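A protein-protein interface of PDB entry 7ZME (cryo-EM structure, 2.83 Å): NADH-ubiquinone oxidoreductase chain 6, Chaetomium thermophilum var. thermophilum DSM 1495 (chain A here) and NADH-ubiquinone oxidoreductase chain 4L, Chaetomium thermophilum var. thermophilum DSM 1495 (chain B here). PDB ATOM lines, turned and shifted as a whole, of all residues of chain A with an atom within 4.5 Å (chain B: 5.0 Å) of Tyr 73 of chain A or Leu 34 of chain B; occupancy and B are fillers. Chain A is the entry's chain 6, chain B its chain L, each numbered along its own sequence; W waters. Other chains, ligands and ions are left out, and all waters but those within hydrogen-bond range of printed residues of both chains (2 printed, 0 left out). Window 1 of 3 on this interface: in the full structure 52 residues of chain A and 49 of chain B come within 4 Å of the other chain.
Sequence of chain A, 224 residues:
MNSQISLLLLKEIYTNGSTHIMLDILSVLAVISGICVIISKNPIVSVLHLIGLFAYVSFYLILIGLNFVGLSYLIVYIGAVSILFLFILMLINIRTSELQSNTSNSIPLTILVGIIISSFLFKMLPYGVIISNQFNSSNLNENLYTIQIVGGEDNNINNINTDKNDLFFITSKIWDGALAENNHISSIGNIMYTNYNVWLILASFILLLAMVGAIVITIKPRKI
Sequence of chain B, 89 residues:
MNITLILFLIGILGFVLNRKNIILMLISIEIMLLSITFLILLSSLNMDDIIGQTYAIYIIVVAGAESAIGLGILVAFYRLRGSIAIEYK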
ATOM      1  N   LEU A  53      36.482  15.373 -32.453  1.00  0.00           N
ATOM      2  CA  LEU A  53      35.901  16.538 -33.113  1.00  0.00           C
ATOM      3  C   LEU A  53      35.166  17.422 -32.116  1.00  0.00           C
ATOM      4  O   LEU A  53      35.272  18.651 -32.162  1.00  0.00           O
ATOM      5  CB  LEU A  53      34.963  16.080 -34.232  1.00  0.00           C
ATOM      6  CG  LEU A  53      33.910  17.035 -34.797  1.00  0.00           C
ATOM      7  CD1 LEU A  53      34.538  18.263 -35.430  1.00  0.00           C
ATOM      8  CD2 LEU A  53      33.042  16.308 -35.800  1.00  0.00           C
ATOM      9  N   PHE A  54      34.415  16.810 -31.204  1.00  0.00           N
ATOM     10  CA  PHE A  54      33.752  17.584 -30.164  1.00  0.00           C
ATOM     11  C   PHE A  54      34.762  18.213 -29.213  1.00  0.00           C
ATOM     12  O   PHE A  54      34.468  19.232 -28.581  1.00  0.00           O
ATOM     13  CB  PHE A  54      32.776  16.697 -29.394  1.00  0.00           C
ATOM     14  CG  PHE A  54      31.490  16.435 -30.121  1.00  0.00           C
ATOM     15  CD1 PHE A  54      30.460  17.347 -30.083  1.00  0.00           C
ATOM     16  CD2 PHE A  54      31.308  15.264 -30.827  1.00  0.00           C
ATOM     17  CE1 PHE A  54      29.278  17.107 -30.747  1.00  0.00           C
ATOM     18  CE2 PHE A  54      30.127  15.017 -31.492  1.00  0.00           C
ATOM     19  CZ  PHE A  54      29.113  15.939 -31.453  1.00  0.00           C
ATOM     20  N   VAL A  57      36.306  21.522 -30.761  1.00  0.00           N
ATOM     21  CA  VAL A  57      35.298  22.572 -30.719  1.00  0.00           C
ATOM     22  C   VAL A  57      35.122  23.079 -29.298  1.00  0.00           C
ATOM     23  O   VAL A  57      34.977  24.285 -29.076  1.00  0.00           O
ATOM     24  CB  VAL A  57      33.975  22.061 -31.319  1.00  0.00           C
ATOM     25  CG1 VAL A  57      32.834  23.015 -30.991  1.00  0.00           C
ATOM     26  CG2 VAL A  57      34.113  21.892 -32.820  1.00  0.00           C
ATOM     27  N   SER A  58      35.143  22.181 -28.315  1.00  0.00           N
ATOM     28  CA  SER A  58      35.066  22.585 -26.919  1.00  0.00           C
ATOM     29  C   SER A  58      36.287  23.379 -26.481  1.00  0.00           C
ATOM     30  O   SER A  58      36.150  24.356 -25.740  1.00  0.00           O
ATOM     31  CB  SER A  58      34.892  21.358 -26.030  1.00  0.00           C
ATOM     32  OG  SER A  58      33.651  20.732 -26.290  1.00  0.00           O
ATOM     33  N   LEU A  61      35.881  26.773 -27.852  1.00  0.00           N
ATOM     34  CA  LEU A  61      34.954  27.582 -27.070  1.00  0.00           C
ATOM     35  C   LEU A  61      35.571  28.029 -25.753  1.00  0.00           C
ATOM     36  O   LEU A  61      35.391  29.178 -25.342  1.00  0.00           O
ATOM     37  CB  LEU A  61      33.666  26.804 -26.813  1.00  0.00           C
ATOM     38  CG  LEU A  61      32.824  26.468 -28.041  1.00  0.00           C
ATOM     39  CD1 LEU A  61      31.913  25.298 -27.742  1.00  0.00           C
ATOM     40  CD2 LEU A  61      32.028  27.672 -28.493  1.00  0.00           C
ATOM     41  N   VAL A  69      29.689  26.559 -21.551  1.00  0.00           N
ATOM     42  CA  VAL A  69      29.142  25.813 -22.709  1.00  0.00           C
ATOM     43  C   VAL A  69      30.253  24.923 -23.283  1.00  0.00           C
ATOM     44  O   VAL A  69      29.932  23.881 -23.801  1.00  0.00           O
ATOM     45  CB  VAL A  69      28.497  26.799 -23.713  1.00  0.00           C
ATOM     46  CG1 VAL A  69      29.514  27.658 -24.444  1.00  0.00           C
ATOM     47  CG2 VAL A  69      27.556  26.106 -24.684  1.00  0.00           C
ATOM     48  N   GLY A  70      31.510  25.348 -23.223  1.00  0.00           N
ATOM     49  CA  GLY A  70      32.632  24.512 -23.681  1.00  0.00           C
ATOM     50  C   GLY A  70      32.856  23.321 -22.772  1.00  0.00           C
ATOM     51  O   GLY A  70      33.077  22.228 -23.299  1.00  0.00           O
ATOM     52  N   LEU A  71      32.811  23.512 -21.453  1.00  0.00           N
ATOM     53  CA  LEU A  71      32.960  22.339 -20.600  1.00  0.00           C
ATOM     54  C   LEU A  71      31.699  21.489 -20.605  1.00  0.00           C
ATOM     55  O   LEU A  71      31.775  20.256 -20.622  1.00  0.00           O
ATOM     56  CB  LEU A  71      33.304  22.767 -19.176  1.00  0.00           C
ATOM     57  CG  LEU A  71      34.745  23.172 -18.891  1.00  0.00           C
ATOM     58  CD1 LEU A  71      34.858  23.690 -17.473  1.00  0.00           C
ATOM     59  CD2 LEU A  71      35.688  22.007 -19.116  1.00  0.00           C
ATOM     60  N   SER A  72      30.552  22.138 -20.740  1.00  0.00           N
ATOM     61  CA  SER A  72      29.249  21.433 -20.744  1.00  0.00           C
ATOM     62  C   SER A  72      29.087  20.632 -22.024  1.00  0.00           C
ATOM     63  O   SER A  72      28.544  19.528 -21.928  1.00  0.00           O
ATOM     64  CB  SER A  72      28.145  22.410 -20.554  1.00  0.00           C
ATOM     65  OG  SER A  72      28.227  22.958 -19.254  1.00  0.00           O
ATOM     66  N   TYR A  73      29.542  21.169 -23.156  1.00  0.00           N
ATOM     67  CA  TYR A  73      29.535  20.411 -24.429  1.00  0.00           C
ATOM     68  C   TYR A  73      30.344  19.137 -24.243  1.00  0.00           C
ATOM     69  O   TYR A  73      29.851  18.059 -24.554  1.00  0.00           O
ATOM     70  CB  TYR A  73      30.208  21.217 -25.544  1.00  0.00           C
ATOM     71  CG  TYR A  73      29.416  21.297 -26.820  1.00  0.00           C
ATOM     72  CD1 TYR A  73      28.714  22.440 -27.147  1.00  0.00           C
ATOM     73  CD2 TYR A  73      29.346  20.223 -27.687  1.00  0.00           C
ATOM     74  CE1 TYR A  73      27.968  22.518 -28.309  1.00  0.00           C
ATOM     75  CE2 TYR A  73      28.606  20.283 -28.854  1.00  0.00           C
ATOM     76  CZ  TYR A  73      27.919  21.439 -29.170  1.00  0.00           C
ATOM     77  OH  TYR A  73      27.192  21.513 -30.320  1.00  0.00           O
ATOM     78  N   LEU A  74      31.560  19.279 -23.743  1.00  0.00           N
ATOM     79  CA  LEU A  74      32.460  18.111 -23.569  1.00  0.00           C
ATOM     80  C   LEU A  74      31.792  17.105 -22.632  1.00  0.00           C
ATOM     81  O   LEU A  74      31.616  15.970 -23.058  1.00  0.00           O
ATOM     82  CB  LEU A  74      33.781  18.621 -22.978  1.00  0.00           C
ATOM     83  CG  LEU A  74      35.036  17.810 -23.275  1.00  0.00           C
ATOM     84  CD1 LEU A  74      35.267  17.692 -24.773  1.00  0.00           C
ATOM     85  CD2 LEU A  74      36.239  18.440 -22.598  1.00  0.00           C
ATOM     86  N   ILE A  75      31.280  17.552 -21.491  1.00  0.00           N
ATOM     87  CA  ILE A  75      30.666  16.629 -20.485  1.00  0.00           C
ATOM     88  C   ILE A  75      29.522  15.862 -21.129  1.00  0.00           C
ATOM     89  O   ILE A  75      29.485  14.637 -20.990  1.00  0.00           O
ATOM     90  CB  ILE A  75      30.168  17.390 -19.239  1.00  0.00           C
ATOM     91  CG1 ILE A  75      31.325  17.812 -18.331  1.00  0.00           C
ATOM     92  CG2 ILE A  75      29.129  16.588 -18.476  1.00  0.00           C
ATOM     93  CD1 ILE A  75      30.931  18.804 -17.270  1.00  0.00           C
ATOM     94  N   VAL A  76      28.656  16.561 -21.845  1.00  0.00           N
ATOM     95  CA  VAL A  76      27.472  15.882 -22.357  1.00  0.00           C
ATOM     96  C   VAL A  76      27.850  14.856 -23.418  1.00  0.00           C
ATOM     97  O   VAL A  76      27.297  13.751 -23.461  1.00  0.00           O
ATOM     98  CB  VAL A  76      26.467  16.917 -22.895  1.00  0.00           C
ATOM     99  CG1 VAL A  76      25.477  16.269 -23.847  1.00  0.00           C
ATOM    100  CG2 VAL A  76      25.747  17.572 -21.747  1.00  0.00           C
ATOM    101  N   TYR A  77      28.773  15.219 -24.301  1.00  0.00           N
ATOM    102  CA  TYR A  77      29.104  14.363 -25.467  1.00  0.00           C
ATOM    103  C   TYR A  77      30.058  13.220 -25.141  1.00  0.00           C
ATOM    104  O   TYR A  77      30.022  12.238 -25.861  1.00  0.00           O
ATOM    105  CB  TYR A  77      29.467  15.244 -26.665  1.00  0.00           C
ATOM    106  CG  TYR A  77      28.233  15.910 -27.208  1.00  0.00           C
ATOM    107  CD1 TYR A  77      27.284  15.173 -27.886  1.00  0.00           C
ATOM    108  CD2 TYR A  77      27.962  17.241 -26.954  1.00  0.00           C
ATOM    109  CE1 TYR A  77      26.115  15.755 -28.337  1.00  0.00           C
ATOM    110  CE2 TYR A  77      26.802  17.841 -27.410  1.00  0.00           C
ATOM    111  CZ  TYR A  77      25.877  17.096 -28.113  1.00  0.00           C
ATOM    112  OH  TYR A  77      24.728  17.667 -28.576  1.00  0.00           O
ATOM    113  N   LEU B   7      32.036  22.479 -41.186  1.00  0.00           N
ATOM    114  CA  LEU B   7      31.481  21.382 -40.404  1.00  0.00           C
ATOM    115  C   LEU B   7      30.078  21.021 -40.864  1.00  0.00           C
ATOM    116  O   LEU B   7      29.715  19.839 -40.884  1.00  0.00           O
ATOM    117  CB  LEU B   7      31.477  21.730 -38.916  1.00  0.00           C
ATOM    118  CG  LEU B   7      32.817  21.899 -38.210  1.00  0.00           C
ATOM    119  CD1 LEU B   7      32.595  22.373 -36.792  1.00  0.00           C
ATOM    120  CD2 LEU B   7      33.601  20.601 -38.224  1.00  0.00           C
ATOM    121  N   GLU B  30      24.294  14.767 -35.801  1.00  0.00           N
ATOM    122  CA  GLU B  30      24.964  15.353 -34.646  1.00  0.00           C
ATOM    123  C   GLU B  30      25.989  16.396 -35.069  1.00  0.00           C
ATOM    124  O   GLU B  30      26.117  17.446 -34.431  1.00  0.00           O
ATOM    125  CB  GLU B  30      25.643  14.258 -33.829  1.00  0.00           C
ATOM    126  CG  GLU B  30      24.714  13.423 -32.983  1.00  0.00           C
ATOM    127  CD  GLU B  30      25.465  12.424 -32.131  1.00  0.00           C
ATOM    128  OE1 GLU B  30      26.577  12.022 -32.532  1.00  0.00           O
ATOM    129  OE2 GLU B  30      24.946  12.041 -31.061  1.00  0.00           O
ATOM    130  N   ILE B  31      26.739  16.115 -36.134  1.00  0.00           N
ATOM    131  CA  ILE B  31      27.750  17.054 -36.608  1.00  0.00           C
ATOM    132  C   ILE B  31      27.099  18.342 -37.096  1.00  0.00           C
ATOM    133  O   ILE B  31      27.600  19.442 -36.840  1.00  0.00           O
ATOM    134  CB  ILE B  31      28.610  16.395 -37.702  1.00  0.00           C
ATOM    135  CG1 ILE B  31      29.430  15.249 -37.114  1.00  0.00           C
ATOM    136  CG2 ILE B  31      29.519  17.415 -38.365  1.00  0.00           C
ATOM    137  CD1 ILE B  31      30.202  14.466 -38.149  1.00  0.00           C
ATOM    138  N   MET B  32      25.981  18.227 -37.815  1.00  0.00           N
ATOM    139  CA  MET B  32      25.291  19.415 -38.307  1.00  0.00           C
ATOM    140  C   MET B  32      24.792  20.282 -37.160  1.00  0.00           C
ATOM    141  O   MET B  32      24.934  21.509 -37.194  1.00  0.00           O
ATOM    142  CB  MET B  32      24.128  19.010 -39.207  1.00  0.00           C
ATOM    143  CG  MET B  32      24.552  18.330 -40.478  1.00  0.00           C
ATOM    144  SD  MET B  32      23.257  18.296 -41.714  1.00  0.00           S
ATOM    145  CE  MET B  32      22.693  16.611 -41.545  1.00  0.00           C
ATOM    146  N   LEU B  33      24.201  19.660 -36.140  1.00  0.00           N
ATOM    147  CA  LEU B  33      23.749  20.411 -34.979  1.00  0.00           C
ATOM    148  C   LEU B  33      24.918  21.055 -34.249  1.00  0.00           C
ATOM    149  O   LEU B  33      24.783  22.167 -33.728  1.00  0.00           O
ATOM    150  CB  LEU B  33      22.960  19.497 -34.045  1.00  0.00           C
ATOM    151  CG  LEU B  33      21.663  18.951 -34.648  1.00  0.00           C
ATOM    152  CD1 LEU B  33      20.817  18.262 -33.603  1.00  0.00           C
ATOM    153  CD2 LEU B  33      20.873  20.043 -35.335  1.00  0.00           C
ATOM    154  N   LEU B  34      26.063  20.372 -34.194  1.00  0.00           N
ATOM    155  CA  LEU B  34      27.283  20.987 -33.682  1.00  0.00           C
ATOM    156  C   LEU B  34      27.610  22.276 -34.420  1.00  0.00           C
ATOM    157  O   LEU B  34      27.829  23.316 -33.791  1.00  0.00           O
ATOM    158  CB  LEU B  34      28.447  19.999 -33.794  1.00  0.00           C
ATOM    159  CG  LEU B  34      29.877  20.516 -33.591  1.00  0.00           C
ATOM    160  CD1 LEU B  34      30.046  21.202 -32.267  1.00  0.00           C
ATOM    161  CD2 LEU B  34      30.884  19.388 -33.734  1.00  0.00           C
ATOM    162  N   SER B  35      27.647  22.226 -35.752  1.00  0.00           N
ATOM    163  CA  SER B  35      28.034  23.397 -36.533  1.00  0.00           C
ATOM    164  C   SER B  35      27.036  24.535 -36.370  1.00  0.00           C
ATOM    165  O   SER B  35      27.429  25.701 -36.260  1.00  0.00           O
ATOM    166  CB  SER B  35      28.176  23.016 -38.004  1.00  0.00           C
ATOM    167  OG  SER B  35      26.944  23.161 -38.683  1.00  0.00           O
ATOM    168  N   ILE B  36      25.738  24.218 -36.365  1.00  0.00           N
ATOM    169  CA  ILE B  36      24.721  25.248 -36.186  1.00  0.00           C
ATOM    170  C   ILE B  36      24.830  25.867 -34.800  1.00  0.00           C
ATOM    171  O   ILE B  36      24.767  27.090 -34.646  1.00  0.00           O
ATOM    172  CB  ILE B  36      23.316  24.667 -36.444  1.00  0.00           C
ATOM    173  CG1 ILE B  36      23.189  24.166 -37.884  1.00  0.00           C
ATOM    174  CG2 ILE B  36      22.236  25.694 -36.158  1.00  0.00           C
ATOM    175  CD1 ILE B  36      23.774  25.095 -38.914  1.00  0.00           C
ATOM    176  N   THR B  37      25.000  25.033 -33.772  1.00  0.00           N
ATOM    177  CA  THR B  37      25.198  25.539 -32.417  1.00  0.00           C
ATOM    178  C   THR B  37      26.446  26.407 -32.337  1.00  0.00           C
ATOM    179  O   THR B  37      26.447  27.455 -31.682  1.00  0.00           O
ATOM    180  CB  THR B  37      25.301  24.369 -31.437  1.00  0.00           C
ATOM    181  OG1 THR B  37      24.019  23.757 -31.282  1.00  0.00           O
ATOM    182  CG2 THR B  37      25.797  24.827 -30.084  1.00  0.00           C
ATOM    183  N   PHE B  38      27.510  25.990 -33.019  1.00  0.00           N
ATOM    184  CA  PHE B  38      28.781  26.691 -32.927  1.00  0.00           C
ATOM    185  C   PHE B  38      28.703  28.061 -33.591  1.00  0.00           C
ATOM    186  O   PHE B  38      29.350  29.012 -33.143  1.00  0.00           O
ATOM    187  CB  PHE B  38      29.874  25.815 -33.545  1.00  0.00           C
ATOM    188  CG  PHE B  38      31.264  26.326 -33.339  1.00  0.00           C
ATOM    189  CD1 PHE B  38      31.720  26.629 -32.072  1.00  0.00           C
ATOM    190  CD2 PHE B  38      32.135  26.440 -34.403  1.00  0.00           C
ATOM    191  CE1 PHE B  38      33.002  27.080 -31.878  1.00  0.00           C
ATOM    192  CE2 PHE B  38      33.424  26.886 -34.210  1.00  0.00           C
ATOM    193  CZ  PHE B  38      33.856  27.207 -32.947  1.00  0.00           C
ATOM    194  N   LEU B  39      27.908  28.185 -34.655  1.00  0.00           N
ATOM    195  CA  LEU B  39      27.687  29.496 -35.259  1.00  0.00           C
ATOM    196  C   LEU B  39      26.928  30.418 -34.315  1.00  0.00           C
ATOM    197  O   LEU B  39      27.244  31.609 -34.212  1.00  0.00           O
ATOM    198  CB  LEU B  39      26.934  29.348 -36.579  1.00  0.00           C
ATOM    199  CG  LEU B  39      26.468  30.663 -37.204  1.00  0.00           C
ATOM    200  CD1 LEU B  39      27.642  31.429 -37.771  1.00  0.00           C
ATOM    201  CD2 LEU B  39      25.414  30.419 -38.263  1.00  0.00           C
ATOM    202  N   LEU B  41      26.954  30.316 -31.087  1.00  0.00           N
ATOM    203  CA  LEU B  41      27.831  30.655 -29.933  1.00  0.00           C
ATOM    204  C   LEU B  41      28.775  31.798 -30.285  1.00  0.00           C
ATOM    205  O   LEU B  41      28.914  32.712 -29.464  1.00  0.00           O
ATOM    206  CB  LEU B  41      28.566  29.420 -29.414  1.00  0.00           C
ATOM    207  CG  LEU B  41      27.693  28.467 -28.600  1.00  0.00           C
ATOM    208  CD1 LEU B  41      28.402  27.153 -28.333  1.00  0.00           C
ATOM    209  CD2 LEU B  41      27.255  29.113 -27.298  1.00  0.00           C
ATOM    210  N   ILE B  60      21.484  21.555 -27.559  1.00  0.00           N
ATOM    211  CA  ILE B  60      22.210  20.387 -27.074  1.00  0.00           C
ATOM    212  C   ILE B  60      21.259  19.399 -26.411  1.00  0.00           C
ATOM    213  O   ILE B  60      21.409  18.182 -26.559  1.00  0.00           O
ATOM    214  CB  ILE B  60      23.335  20.828 -26.120  1.00  0.00           C
ATOM    215  CG1 ILE B  60      24.371  21.661 -26.873  1.00  0.00           C
ATOM    216  CG2 ILE B  60      24.003  19.627 -25.479  1.00  0.00           C
ATOM    217  CD1 ILE B  60      25.065  22.693 -26.011  1.00  0.00           C
HETATM  218  O   HOH W   1      23.313  15.974 -26.409  1.00  0.00           O
HETATM  219  O   HOH W   2      26.012  16.213 -31.190  1.00  0.00           O
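Tyr 73 of chain A touches just these residues of chain B: Leu 34, Thr 37 and Ile 60. Leu 34 of chain B touches just these residues of chain A: Leu 53 (3.98 Å), Val 57 (3.6 Å) and Tyr 73 (3.4 Å). Printed residues of chain B within 4 Å of Leu 61 of chain A: Phe 38 and Leu 41. Printed residues of chain A within 4 Å of Leu 7 of chain B: Leu 53. Leu 39 of chain B touches none of the printed residues of chain A. The nearest residue of chain A that does not touch Leu 34 of chain B is Phe 54 of chain A (4.1 Å). The nearest printed residue of chain A that does not touch Leu 7 of chain B is Val 57 of chain A (4.3 Å).
Water W1 bridges O of Ile 60 of chain B (2.9 Å) and OH of Tyr 77 of chain A (3.1 Å). Water W2 lies within hydrogen-bond range of the side-chain hydroxyl (OH) of Tyr 77 of chain A (3.3 Å) and the backbone carbonyl oxygen (O) of Glu 30 of chain B (3.5 Å).
Hydrophobic or aromatic side chains of chain A within 4 Å of the printed part of chain B: Leu 53, Val 57, Leu 61, Val 69, Tyr 73 and Tyr 77.
Among the printed residues, pairs that only touch across the chains: Leu 53 of chain A with Leu 7 of chain B, Leu 53 of chain A with Ile 31 of chain B, Leu 53 of chain A with Leu 34 of chain B, Val 57 of chain A with Leu 34 of chain B, Val 57 of chain A with Phe 38 of chain B, Leu 61 of chain A with Phe 38 of chain B, Leu 61 of chain A with Leu 41 of chain B, Val 69 of chain A with Leu 41 of chain B, Tyr 73 of chain A with Leu 34 of chain B, Tyr 73 of chain A with Thr 37 of chain B, Tyr 73 of chain A with Ile 60 of chain B and Tyr 77 of chain A with Ile 60 of chain B.
O of Leu 33 of chain B sits at hydrogen-bond distance from OG1 of Thr 37 of chain B (3.0 Å).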
